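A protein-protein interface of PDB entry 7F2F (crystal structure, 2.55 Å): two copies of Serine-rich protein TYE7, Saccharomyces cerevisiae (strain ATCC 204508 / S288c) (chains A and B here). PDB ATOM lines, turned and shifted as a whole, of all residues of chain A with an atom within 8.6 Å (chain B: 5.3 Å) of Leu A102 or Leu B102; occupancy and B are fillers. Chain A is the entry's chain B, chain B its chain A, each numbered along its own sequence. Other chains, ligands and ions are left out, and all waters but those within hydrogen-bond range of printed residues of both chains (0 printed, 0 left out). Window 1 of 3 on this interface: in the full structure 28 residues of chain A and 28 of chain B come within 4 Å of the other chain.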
ATOM      1  N   ILE A  43       0.634   1.592  16.749  1.00  0.00           N
ATOM      2  CA  ILE A  43      -0.063   0.522  16.023  1.00  0.00           C
ATOM      3  C   ILE A  43       0.811  -0.676  15.824  1.00  0.00           C
ATOM      4  O   ILE A  43       0.326  -1.679  15.382  1.00  0.00           O
ATOM      5  CB  ILE A  43      -0.628   0.923  14.637  1.00  0.00           C
ATOM      6  CG1 ILE A  43       0.382   1.702  13.845  1.00  0.00           C
ATOM      7  CG2 ILE A  43      -1.873   1.754  14.783  1.00  0.00           C
ATOM      8  CD1 ILE A  43       0.073   1.569  12.406  1.00  0.00           C
ATOM      9  N   ILE A  44       2.089  -0.574  16.158  1.00  0.00           N
ATOM     10  CA  ILE A  44       2.994  -1.712  16.077  1.00  0.00           C
ATOM     11  C   ILE A  44       2.945  -2.446  17.395  1.00  0.00           C
ATOM     12  O   ILE A  44       3.392  -1.909  18.363  1.00  0.00           O
ATOM     13  CB  ILE A  44       4.410  -1.237  15.834  1.00  0.00           C
ATOM     14  CG1 ILE A  44       4.478  -0.484  14.505  1.00  0.00           C
ATOM     15  CG2 ILE A  44       5.360  -2.422  15.911  1.00  0.00           C
ATOM     16  CD1 ILE A  44       5.734   0.363  14.364  1.00  0.00           C
ATOM     17  N   PRO A  45       2.366  -3.641  17.447  1.00  0.00           N
ATOM     18  CA  PRO A  45       2.248  -4.335  18.741  1.00  0.00           C
ATOM     19  C   PRO A  45       3.574  -4.693  19.410  1.00  0.00           C
ATOM     20  O   PRO A  45       3.618  -4.805  20.603  1.00  0.00           O
ATOM     21  CB  PRO A  45       1.463  -5.621  18.441  1.00  0.00           C
ATOM     22  CG  PRO A  45       1.345  -5.699  16.979  1.00  0.00           C
ATOM     23  CD  PRO A  45       1.781  -4.410  16.340  1.00  0.00           C
ATOM     24  N   TRP A  46       4.632  -4.841  18.650  1.00  0.00           N
ATOM     25  CA  TRP A  46       5.946  -5.051  19.221  1.00  0.00           C
ATOM     26  C   TRP A  46       6.373  -3.947  20.168  1.00  0.00           C
ATOM     27  O   TRP A  46       7.060  -4.250  21.128  1.00  0.00           O
ATOM     28  CB  TRP A  46       6.997  -5.167  18.106  1.00  0.00           C
ATOM     29  CG  TRP A  46       6.687  -6.256  17.191  1.00  0.00           C
ATOM     30  CD1 TRP A  46       5.779  -7.262  17.391  1.00  0.00           C
ATOM     31  CD2 TRP A  46       7.235  -6.451  15.896  1.00  0.00           C
ATOM     32  NE1 TRP A  46       5.736  -8.064  16.275  1.00  0.00           N
ATOM     33  CE2 TRP A  46       6.621  -7.590  15.348  1.00  0.00           C
ATOM     34  CE3 TRP A  46       8.188  -5.781  15.147  1.00  0.00           C
ATOM     35  CZ2 TRP A  46       6.929  -8.077  14.090  1.00  0.00           C
ATOM     36  CZ3 TRP A  46       8.529  -6.288  13.867  1.00  0.00           C
ATOM     37  CH2 TRP A  46       7.892  -7.408  13.360  1.00  0.00           C
ATOM     38  N   ALA A  95       9.150  -0.015  12.470  1.00  0.00           N
ATOM     39  CA  ALA A  95       8.070   0.217  11.536  1.00  0.00           C
ATOM     40  C   ALA A  95       8.370  -0.427  10.259  1.00  0.00           C
ATOM     41  O   ALA A  95       7.540  -1.123   9.700  1.00  0.00           O
ATOM     42  CB  ALA A  95       7.871   1.671  11.319  1.00  0.00           C
ATOM     43  N   VAL A  96       9.550  -0.215   9.747  1.00  0.00           N
ATOM     44  CA  VAL A  96       9.923  -0.974   8.547  1.00  0.00           C
ATOM     45  C   VAL A  96       9.899  -2.477   8.771  1.00  0.00           C
ATOM     46  O   VAL A  96       9.523  -3.192   7.857  1.00  0.00           O
ATOM     47  CB  VAL A  96      11.309  -0.594   8.001  1.00  0.00           C
ATOM     48  CG1 VAL A  96      11.784  -1.599   6.981  1.00  0.00           C
ATOM     49  CG2 VAL A  96      11.262   0.756   7.328  1.00  0.00           C
ATOM     50  N   ASP A  97      10.305  -2.981   9.933  1.00  0.00           N
ATOM     51  CA  ASP A  97      10.417  -4.439  10.013  1.00  0.00           C
ATOM     52  C   ASP A  97       9.024  -4.999  10.129  1.00  0.00           C
ATOM     53  O   ASP A  97       8.733  -6.110   9.616  1.00  0.00           O
ATOM     54  CB  ASP A  97      11.192  -4.918  11.268  1.00  0.00           C
ATOM     55  CG  ASP A  97      12.669  -4.637  11.217  1.00  0.00           C
ATOM     56  OD1 ASP A  97      13.317  -4.692  10.136  1.00  0.00           O
ATOM     57  OD2 ASP A  97      13.184  -4.404  12.312  1.00  0.00           O
ATOM     58  N   TYR A  98       8.168  -4.235  10.838  1.00  0.00           N
ATOM     59  CA  TYR A  98       6.816  -4.693  11.094  1.00  0.00           C
ATOM     60  C   TYR A  98       6.025  -4.737   9.787  1.00  0.00           C
ATOM     61  O   TYR A  98       5.196  -5.593   9.611  1.00  0.00           O
ATOM     62  CB  TYR A  98       6.115  -3.875  12.146  1.00  0.00           C
ATOM     63  CG  TYR A  98       4.694  -4.337  12.398  1.00  0.00           C
ATOM     64  CD1 TYR A  98       4.442  -5.569  12.927  1.00  0.00           C
ATOM     65  CD2 TYR A  98       3.600  -3.530  12.113  1.00  0.00           C
ATOM     66  CE1 TYR A  98       3.152  -5.988  13.195  1.00  0.00           C
ATOM     67  CE2 TYR A  98       2.307  -3.946  12.404  1.00  0.00           C
ATOM     68  CZ  TYR A  98       2.099  -5.187  12.928  1.00  0.00           C
ATOM     69  OH  TYR A  98       0.841  -5.634  13.177  1.00  0.00           O
ATOM     70  N   ILE A  99       6.374  -3.908   8.832  1.00  0.00           N
ATOM     71  CA  ILE A  99       5.722  -3.969   7.558  1.00  0.00           C
ATOM     72  C   ILE A  99       6.240  -5.132   6.765  1.00  0.00           C
ATOM     73  O   ILE A  99       5.467  -5.753   6.047  1.00  0.00           O
ATOM     74  CB  ILE A  99       5.806  -2.586   6.826  1.00  0.00           C
ATOM     75  CG1 ILE A  99       4.874  -1.604   7.524  1.00  0.00           C
ATOM     76  CG2 ILE A  99       5.506  -2.641   5.353  1.00  0.00           C
ATOM     77  CD1 ILE A  99       5.296  -0.160   7.296  1.00  0.00           C
ATOM     78  N   LEU A 100       7.529  -5.424   6.816  1.00  0.00           N
ATOM     79  CA  LEU A 100       8.056  -6.583   6.056  1.00  0.00           C
ATOM     80  C   LEU A 100       7.373  -7.819   6.573  1.00  0.00           C
ATOM     81  O   LEU A 100       6.989  -8.679   5.812  1.00  0.00           O
ATOM     82  CB  LEU A 100       9.518  -6.802   6.302  1.00  0.00           C
ATOM     83  CG  LEU A 100      10.451  -5.880   5.557  1.00  0.00           C
ATOM     84  CD1 LEU A 100      11.868  -6.175   6.048  1.00  0.00           C
ATOM     85  CD2 LEU A 100      10.349  -6.074   4.046  1.00  0.00           C
ATOM     86  N   TYR A 101       7.263  -7.900   7.895  1.00  0.00           N
ATOM     87  CA  TYR A 101       6.550  -8.987   8.513  1.00  0.00           C
ATOM     88  C   TYR A 101       5.142  -9.130   7.945  1.00  0.00           C
ATOM     89  O   TYR A 101       4.772 -10.225   7.593  1.00  0.00           O
ATOM     90  CB  TYR A 101       6.479  -8.689   9.962  1.00  0.00           C
ATOM     91  CG  TYR A 101       5.646  -9.599  10.769  1.00  0.00           C
ATOM     92  CD1 TYR A 101       6.044 -10.906  11.013  1.00  0.00           C
ATOM     93  CD2 TYR A 101       4.517  -9.131  11.400  1.00  0.00           C
ATOM     94  CE1 TYR A 101       5.308 -11.737  11.822  1.00  0.00           C
ATOM     95  CE2 TYR A 101       3.787  -9.948  12.210  1.00  0.00           C
ATOM     96  CZ  TYR A 101       4.188 -11.257  12.389  1.00  0.00           C
ATOM     97  OH  TYR A 101       3.451 -12.043  13.203  1.00  0.00           O
ATOM     98  N   LEU A 102       4.372  -8.016   7.829  1.00  0.00           N
ATOM     99  CA  LEU A 102       2.997  -8.087   7.330  1.00  0.00           C
ATOM    100  C   LEU A 102       2.987  -8.373   5.880  1.00  0.00           C
ATOM    101  O   LEU A 102       2.209  -9.186   5.452  1.00  0.00           O
ATOM    102  CB  LEU A 102       2.160  -6.864   7.664  1.00  0.00           C
ATOM    103  CG  LEU A 102       1.908  -6.604   9.166  1.00  0.00           C
ATOM    104  CD1 LEU A 102       1.255  -5.252   9.315  1.00  0.00           C
ATOM    105  CD2 LEU A 102       1.098  -7.658   9.880  1.00  0.00           C
ATOM    106  N   GLN A 103       3.916  -7.819   5.123  1.00  0.00           N
ATOM    107  CA  GLN A 103       4.051  -8.238   3.722  1.00  0.00           C
ATOM    108  C   GLN A 103       4.399  -9.701   3.574  1.00  0.00           C
ATOM    109  O   GLN A 103       3.815 -10.374   2.744  1.00  0.00           O
ATOM    110  CB  GLN A 103       5.046  -7.381   3.012  1.00  0.00           C
ATOM    111  CG  GLN A 103       4.484  -5.988   2.793  1.00  0.00           C
ATOM    112  CD  GLN A 103       5.444  -4.951   2.236  1.00  0.00           C
ATOM    113  OE1 GLN A 103       6.648  -5.156   2.156  1.00  0.00           O
ATOM    114  NE2 GLN A 103       4.892  -3.793   1.875  1.00  0.00           N
ATOM    115  N   ASN A 104       5.307 -10.216   4.401  1.00  0.00           N
ATOM    116  CA  ASN A 104       5.590 -11.635   4.416  1.00  0.00           C
ATOM    117  C   ASN A 104       4.336 -12.415   4.661  1.00  0.00           C
ATOM    118  O   ASN A 104       4.047 -13.305   3.915  1.00  0.00           O
ATOM    119  CB  ASN A 104       6.560 -12.045   5.507  1.00  0.00           C
ATOM    120  CG  ASN A 104       7.979 -11.783   5.149  1.00  0.00           C
ATOM    121  OD1 ASN A 104       8.357 -11.938   3.990  1.00  0.00           O
ATOM    122  ND2 ASN A 104       8.810 -11.414   6.165  1.00  0.00           N
ATOM    123  N   ASN A 105       3.610 -12.094   5.724  1.00  0.00           N
ATOM    124  CA  ASN A 105       2.417 -12.832   6.070  1.00  0.00           C
ATOM    125  C   ASN A 105       1.411 -12.881   4.958  1.00  0.00           C
ATOM    126  O   ASN A 105       0.786 -13.881   4.776  1.00  0.00           O
ATOM    127  CB  ASN A 105       1.748 -12.230   7.260  1.00  0.00           C
ATOM    128  CG  ASN A 105       2.502 -12.478   8.500  1.00  0.00           C
ATOM    129  OD1 ASN A 105       3.614 -13.057   8.476  1.00  0.00           O
ATOM    130  ND2 ASN A 105       1.927 -12.055   9.620  1.00  0.00           N
ATOM    131  N   GLU A 106       1.307 -11.816   4.186  1.00  0.00           N
ATOM    132  CA  GLU A 106       0.409 -11.810   3.073  1.00  0.00           C
ATOM    133  C   GLU A 106       0.921 -12.838   2.051  1.00  0.00           C
ATOM    134  O   GLU A 106       0.135 -13.590   1.536  1.00  0.00           O
ATOM    135  CB  GLU A 106       0.224 -10.385   2.499  1.00  0.00           C
ATOM    136  CG  GLU A 106      -0.272 -10.286   1.059  1.00  0.00           C
ATOM    137  CD  GLU A 106      -0.326  -8.840   0.510  1.00  0.00           C
ATOM    138  OE1 GLU A 106       0.432  -7.929   1.024  1.00  0.00           O
ATOM    139  OE2 GLU A 106      -1.116  -8.633  -0.479  1.00  0.00           O
ATOM    140  N   ARG A 107       2.215 -12.895   1.768  1.00  0.00           N
ATOM    141  CA  ARG A 107       2.733 -13.953   0.875  1.00  0.00           C
ATOM    142  C   ARG A 107       2.355 -15.324   1.417  1.00  0.00           C
ATOM    143  O   ARG A 107       1.786 -16.115   0.697  1.00  0.00           O
ATOM    144  CB  ARG A 107       4.247 -13.862   0.632  1.00  0.00           C
ATOM    145  CG  ARG A 107       4.686 -12.760  -0.331  1.00  0.00           C
ATOM    146  CD  ARG A 107       6.218 -12.686  -0.530  1.00  0.00           C
ATOM    147  NE  ARG A 107       6.919 -11.862   0.479  1.00  0.00           N
ATOM    148  CZ  ARG A 107       6.968 -10.515   0.505  1.00  0.00           C
ATOM    149  NH1 ARG A 107       7.633  -9.886   1.479  1.00  0.00           N
ATOM    150  NH2 ARG A 107       6.352  -9.772  -0.418  1.00  0.00           N
ATOM    151  N   LEU A 108       2.579 -15.567   2.693  1.00  0.00           N
ATOM    152  CA  LEU A 108       2.178 -16.831   3.316  1.00  0.00           C
ATOM    153  C   LEU A 108       0.687 -17.122   3.238  1.00  0.00           C
ATOM    154  O   LEU A 108       0.294 -18.243   3.024  1.00  0.00           O
ATOM    155  CB  LEU A 108       2.610 -16.892   4.780  1.00  0.00           C
ATOM    156  CG  LEU A 108       4.161 -16.734   4.964  1.00  0.00           C
ATOM    157  CD1 LEU A 108       4.662 -17.020   6.385  1.00  0.00           C
ATOM    158  CD2 LEU A 108       4.952 -17.529   3.931  1.00  0.00           C
ATOM    159  N   TYR A 109      -0.147 -16.111   3.413  1.00  0.00           N
ATOM    160  CA  TYR A 109      -1.569 -16.298   3.271  1.00  0.00           C
ATOM    161  C   TYR A 109      -1.958 -16.606   1.837  1.00  0.00           C
ATOM    162  O   TYR A 109      -2.793 -17.448   1.624  1.00  0.00           O
ATOM    163  CB  TYR A 109      -2.336 -15.095   3.724  1.00  0.00           C
ATOM    164  CG  TYR A 109      -2.635 -15.035   5.179  1.00  0.00           C
ATOM    165  CD1 TYR A 109      -3.442 -15.976   5.780  1.00  0.00           C
ATOM    166  CD2 TYR A 109      -2.207 -13.961   5.949  1.00  0.00           C
ATOM    167  CE1 TYR A 109      -3.779 -15.881   7.127  1.00  0.00           C
ATOM    168  CE2 TYR A 109      -2.523 -13.874   7.293  1.00  0.00           C
ATOM    169  CZ  TYR A 109      -3.299 -14.846   7.868  1.00  0.00           C
ATOM    170  OH  TYR A 109      -3.606 -14.717   9.198  1.00  0.00           O
ATOM    171  N   ASP B  97      -1.494   4.527   7.636  1.00  0.00           N
ATOM    172  CA  ASP B  97      -2.627   4.083   6.818  1.00  0.00           C
ATOM    173  C   ASP B  97      -2.360   2.673   6.309  1.00  0.00           C
ATOM    174  O   ASP B  97      -3.196   1.813   6.366  1.00  0.00           O
ATOM    175  CB  ASP B  97      -2.988   5.031   5.682  1.00  0.00           C
ATOM    176  CG  ASP B  97      -3.462   6.416   6.192  1.00  0.00           C
ATOM    177  OD1 ASP B  97      -4.035   6.441   7.309  1.00  0.00           O
ATOM    178  OD2 ASP B  97      -3.265   7.475   5.496  1.00  0.00           O
ATOM    179  N   TYR B  98      -1.153   2.435   5.916  1.00  0.00           N
ATOM    180  CA  TYR B  98      -0.860   1.203   5.240  1.00  0.00           C
ATOM    181  C   TYR B  98      -0.769   0.029   6.225  1.00  0.00           C
ATOM    182  O   TYR B  98      -1.097  -1.092   5.873  1.00  0.00           O
ATOM    183  CB  TYR B  98       0.423   1.380   4.453  1.00  0.00           C
ATOM    184  CG  TYR B  98       0.850   0.185   3.693  1.00  0.00           C
ATOM    185  CD1 TYR B  98       0.175  -0.231   2.569  1.00  0.00           C
ATOM    186  CD2 TYR B  98       1.988  -0.497   4.067  1.00  0.00           C
ATOM    187  CE1 TYR B  98       0.635  -1.325   1.838  1.00  0.00           C
ATOM    188  CE2 TYR B  98       2.437  -1.595   3.379  1.00  0.00           C
ATOM    189  CZ  TYR B  98       1.768  -2.001   2.268  1.00  0.00           C
ATOM    190  OH  TYR B  98       2.273  -3.088   1.652  1.00  0.00           O
ATOM    191  N   ILE B  99      -0.354   0.291   7.450  1.00  0.00           N
ATOM    192  CA  ILE B  99      -0.358  -0.763   8.444  1.00  0.00           C
ATOM    193  C   ILE B  99      -1.780  -1.150   8.851  1.00  0.00           C
ATOM    194  O   ILE B  99      -2.067  -2.330   9.001  1.00  0.00           O
ATOM    195  CB  ILE B  99       0.549  -0.419   9.655  1.00  0.00           C
ATOM    196  CG1 ILE B  99       2.006  -0.478   9.207  1.00  0.00           C
ATOM    197  CG2 ILE B  99       0.405  -1.403  10.790  1.00  0.00           C
ATOM    198  CD1 ILE B  99       2.900   0.355  10.126  1.00  0.00           C
ATOM    199  N   LEU B 100      -2.663  -0.195   9.049  1.00  0.00           N
ATOM    200  CA  LEU B 100      -4.079  -0.512   9.267  1.00  0.00           C
ATOM    201  C   LEU B 100      -4.732  -1.340   8.117  1.00  0.00           C
ATOM    202  O   LEU B 100      -5.417  -2.339   8.328  1.00  0.00           O
ATOM    203  CB  LEU B 100      -4.852   0.784   9.409  1.00  0.00           C
ATOM    204  CG  LEU B 100      -4.569   1.592  10.665  1.00  0.00           C
ATOM    205  CD1 LEU B 100      -5.574   2.724  10.738  1.00  0.00           C
ATOM    206  CD2 LEU B 100      -4.651   0.733  11.923  1.00  0.00           C
ATOM    207  N   TYR B 101      -4.493  -0.910   6.907  1.00  0.00           N
ATOM    208  CA  TYR B 101      -4.887  -1.644   5.741  1.00  0.00           C
ATOM    209  C   TYR B 101      -4.424  -3.075   5.824  1.00  0.00           C
ATOM    210  O   TYR B 101      -5.243  -3.988   5.689  1.00  0.00           O
ATOM    211  CB  TYR B 101      -4.276  -0.955   4.539  1.00  0.00           C
ATOM    212  CG  TYR B 101      -4.410  -1.631   3.241  1.00  0.00           C
ATOM    213  CD1 TYR B 101      -5.644  -1.728   2.602  1.00  0.00           C
ATOM    214  CD2 TYR B 101      -3.293  -2.203   2.640  1.00  0.00           C
ATOM    215  CE1 TYR B 101      -5.755  -2.368   1.383  1.00  0.00           C
ATOM    216  CE2 TYR B 101      -3.380  -2.840   1.420  1.00  0.00           C
ATOM    217  CZ  TYR B 101      -4.607  -2.922   0.798  1.00  0.00           C
ATOM    218  OH  TYR B 101      -4.641  -3.570  -0.395  1.00  0.00           O
ATOM    219  N   LEU B 102      -3.141  -3.284   6.101  1.00  0.00           N
ATOM    220  CA  LEU B 102      -2.598  -4.645   6.114  1.00  0.00           C
ATOM    221  C   LEU B 102      -3.120  -5.431   7.288  1.00  0.00           C
ATOM    222  O   LEU B 102      -3.493  -6.581   7.117  1.00  0.00           O
ATOM    223  CB  LEU B 102      -1.100  -4.660   6.202  1.00  0.00           C
ATOM    224  CG  LEU B 102      -0.316  -4.118   5.010  1.00  0.00           C
ATOM    225  CD1 LEU B 102       1.150  -4.070   5.381  1.00  0.00           C
ATOM    226  CD2 LEU B 102      -0.489  -4.913   3.740  1.00  0.00           C
ATOM    227  N   GLN B 103      -3.211  -4.827   8.469  1.00  0.00           N
ATOM    228  CA  GLN B 103      -3.829  -5.552   9.583  1.00  0.00           C
ATOM    229  C   GLN B 103      -5.263  -5.961   9.324  1.00  0.00           C
ATOM    230  O   GLN B 103      -5.665  -7.080   9.685  1.00  0.00           O
ATOM    231  CB  GLN B 103      -3.781  -4.788  10.858  1.00  0.00           C
ATOM    232  CG  GLN B 103      -2.365  -4.587  11.389  1.00  0.00           C
ATOM    233  CD  GLN B 103      -2.276  -3.481  12.420  1.00  0.00           C
ATOM    234  OE1 GLN B 103      -3.090  -2.567  12.448  1.00  0.00           O
ATOM    235  NE2 GLN B 103      -1.259  -3.546  13.237  1.00  0.00           N
ATOM    236  N   ASN B 104      -6.018  -5.063   8.690  1.00  0.00           N
ATOM    237  CA  ASN B 104      -7.376  -5.333   8.287  1.00  0.00           C
ATOM    238  C   ASN B 104      -7.414  -6.406   7.242  1.00  0.00           C
ATOM    239  O   ASN B 104      -8.147  -7.351   7.433  1.00  0.00           O
ATOM    240  CB  ASN B 104      -8.065  -4.082   7.798  1.00  0.00           C
ATOM    241  CG  ASN B 104      -8.543  -3.185   8.935  1.00  0.00           C
ATOM    242  OD1 ASN B 104      -8.583  -3.565  10.096  1.00  0.00           O
ATOM    243  ND2 ASN B 104      -8.946  -1.978   8.574  1.00  0.00           N
ATOM    244  N   ASN B 105      -6.598  -6.335   6.177  1.00  0.00           N
ATOM    245  CA  ASN B 105      -6.586  -7.478   5.300  1.00  0.00           C
ATOM    246  C   ASN B 105      -6.282  -8.838   5.948  1.00  0.00           C
ATOM    247  O   ASN B 105      -6.852  -9.804   5.520  1.00  0.00           O
ATOM    248  CB  ASN B 105      -5.646  -7.291   4.150  1.00  0.00           C
ATOM    249  CG  ASN B 105      -6.061  -6.191   3.286  1.00  0.00           C
ATOM    250  OD1 ASN B 105      -7.212  -5.822   3.311  1.00  0.00           O
ATOM    251  ND2 ASN B 105      -5.123  -5.610   2.546  1.00  0.00           N
ATOM    252  N   GLU B 106      -5.463  -8.938   6.984  1.00  0.00           N
ATOM    253  CA  GLU B 106      -5.188 -10.273   7.493  1.00  0.00           C
ATOM    254  C   GLU B 106      -6.451 -10.881   8.008  1.00  0.00           C
ATOM    255  O   GLU B 106      -6.644 -12.097   7.882  1.00  0.00           O
ATOM    256  CB  GLU B 106      -4.206 -10.279   8.624  1.00  0.00           C
ATOM    257  CG  GLU B 106      -2.809  -9.943   8.212  1.00  0.00           C
ATOM    258  CD  GLU B 106      -1.804 -10.182   9.324  1.00  0.00           C
ATOM    259  OE1 GLU B 106      -2.099  -9.870  10.514  1.00  0.00           O
ATOM    260  OE2 GLU B 106      -0.707 -10.650   8.988  1.00  0.00           O
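O of Tyr A101 lies close to OD1 of Asn A105 (3.2 Å).
Tyr A98 touches Ile B99, and with the chains exchanged Ile A99 touches Tyr B98. Ile B99 touches its own counterpart, Ile A99. Leu A102 touches its own counterpart, Leu B102. Asn A105 touches Glu B106, but with the chains exchanged Glu A106 does not touch Asn B105 (5.9 Å). Positions printed for both chains: 97, 98, 99, 100, 101, 102, 103, 104, 105 and 106.
NE2 of Gln B103 is in hydrogen-bond range of OH of Tyr A98, 3.0 Å away. The side-chain carboxylate (OE2) of Glu B106 sits at hydrogen-bond distance from the side-chain amide nitrogen (ND2) of Asn A105. The backbone carbonyl oxygen (O) of Ile A43 sits at hydrogen-bond distance from the side-chain amide nitrogen (NE2) of Gln B103 (3.3 Å). The side-chain hydroxyl (OH) of Tyr B98 is in hydrogen-bond range of the side-chain amide nitrogen (NE2) of Gln A103 (2.7 Å).
Among the printed residues, pairs that only touch across the chains: Ile A43 with Ile B99, Tyr A98 with Ile B99, Ile A99 with Tyr B98, Ile A99 with Ile B99, Leu A102 with Leu B102 and Leu A102 with Glu B106.
Hydrophobic or aromatic side chains of chain B within 4 Å of the printed part of chain A: Tyr B98, Ile B99 and Leu B102. Along chain B the printed residues that touch a printed residue of chain A span positions 98 to 106. Of the 19 printed residues of chain A, 6 touch a printed residue of chain B. Printed residues of chain A that touch a printed residue of chain B: Ile A43, Tyr A98, Ile A99, Leu A102, Gln A103 and Asn A105. Among the printed residues, no Asp or Glu carboxylate lies within 4 Å of a Lys or Arg side-chain nitrogen of the other chain.
Of the printed residues of chain B, Tyr A98 touches Ile B99 and Gln B103. Printed residues of chain B within 4 Å of Leu A102: Leu B102 and Glu B106. Printed residues of chain B within 4 Å of Gln A103: Tyr B98 (2.7 Å). Glu A106 touches none of the printed residues of chain B. Of chain A, only Leu A102 (3.7 Å) comes within 4 Å of Leu B102. Of the printed residues of chain A, Gln B103 touches Ile A43 and Tyr A98. The nearest printed residue of chain B that does not touch Leu A102 is Ile B99 (4.2 Å). The nearest residue of chain A that does not touch Leu B102 is Glu A106 (4.2 Å).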
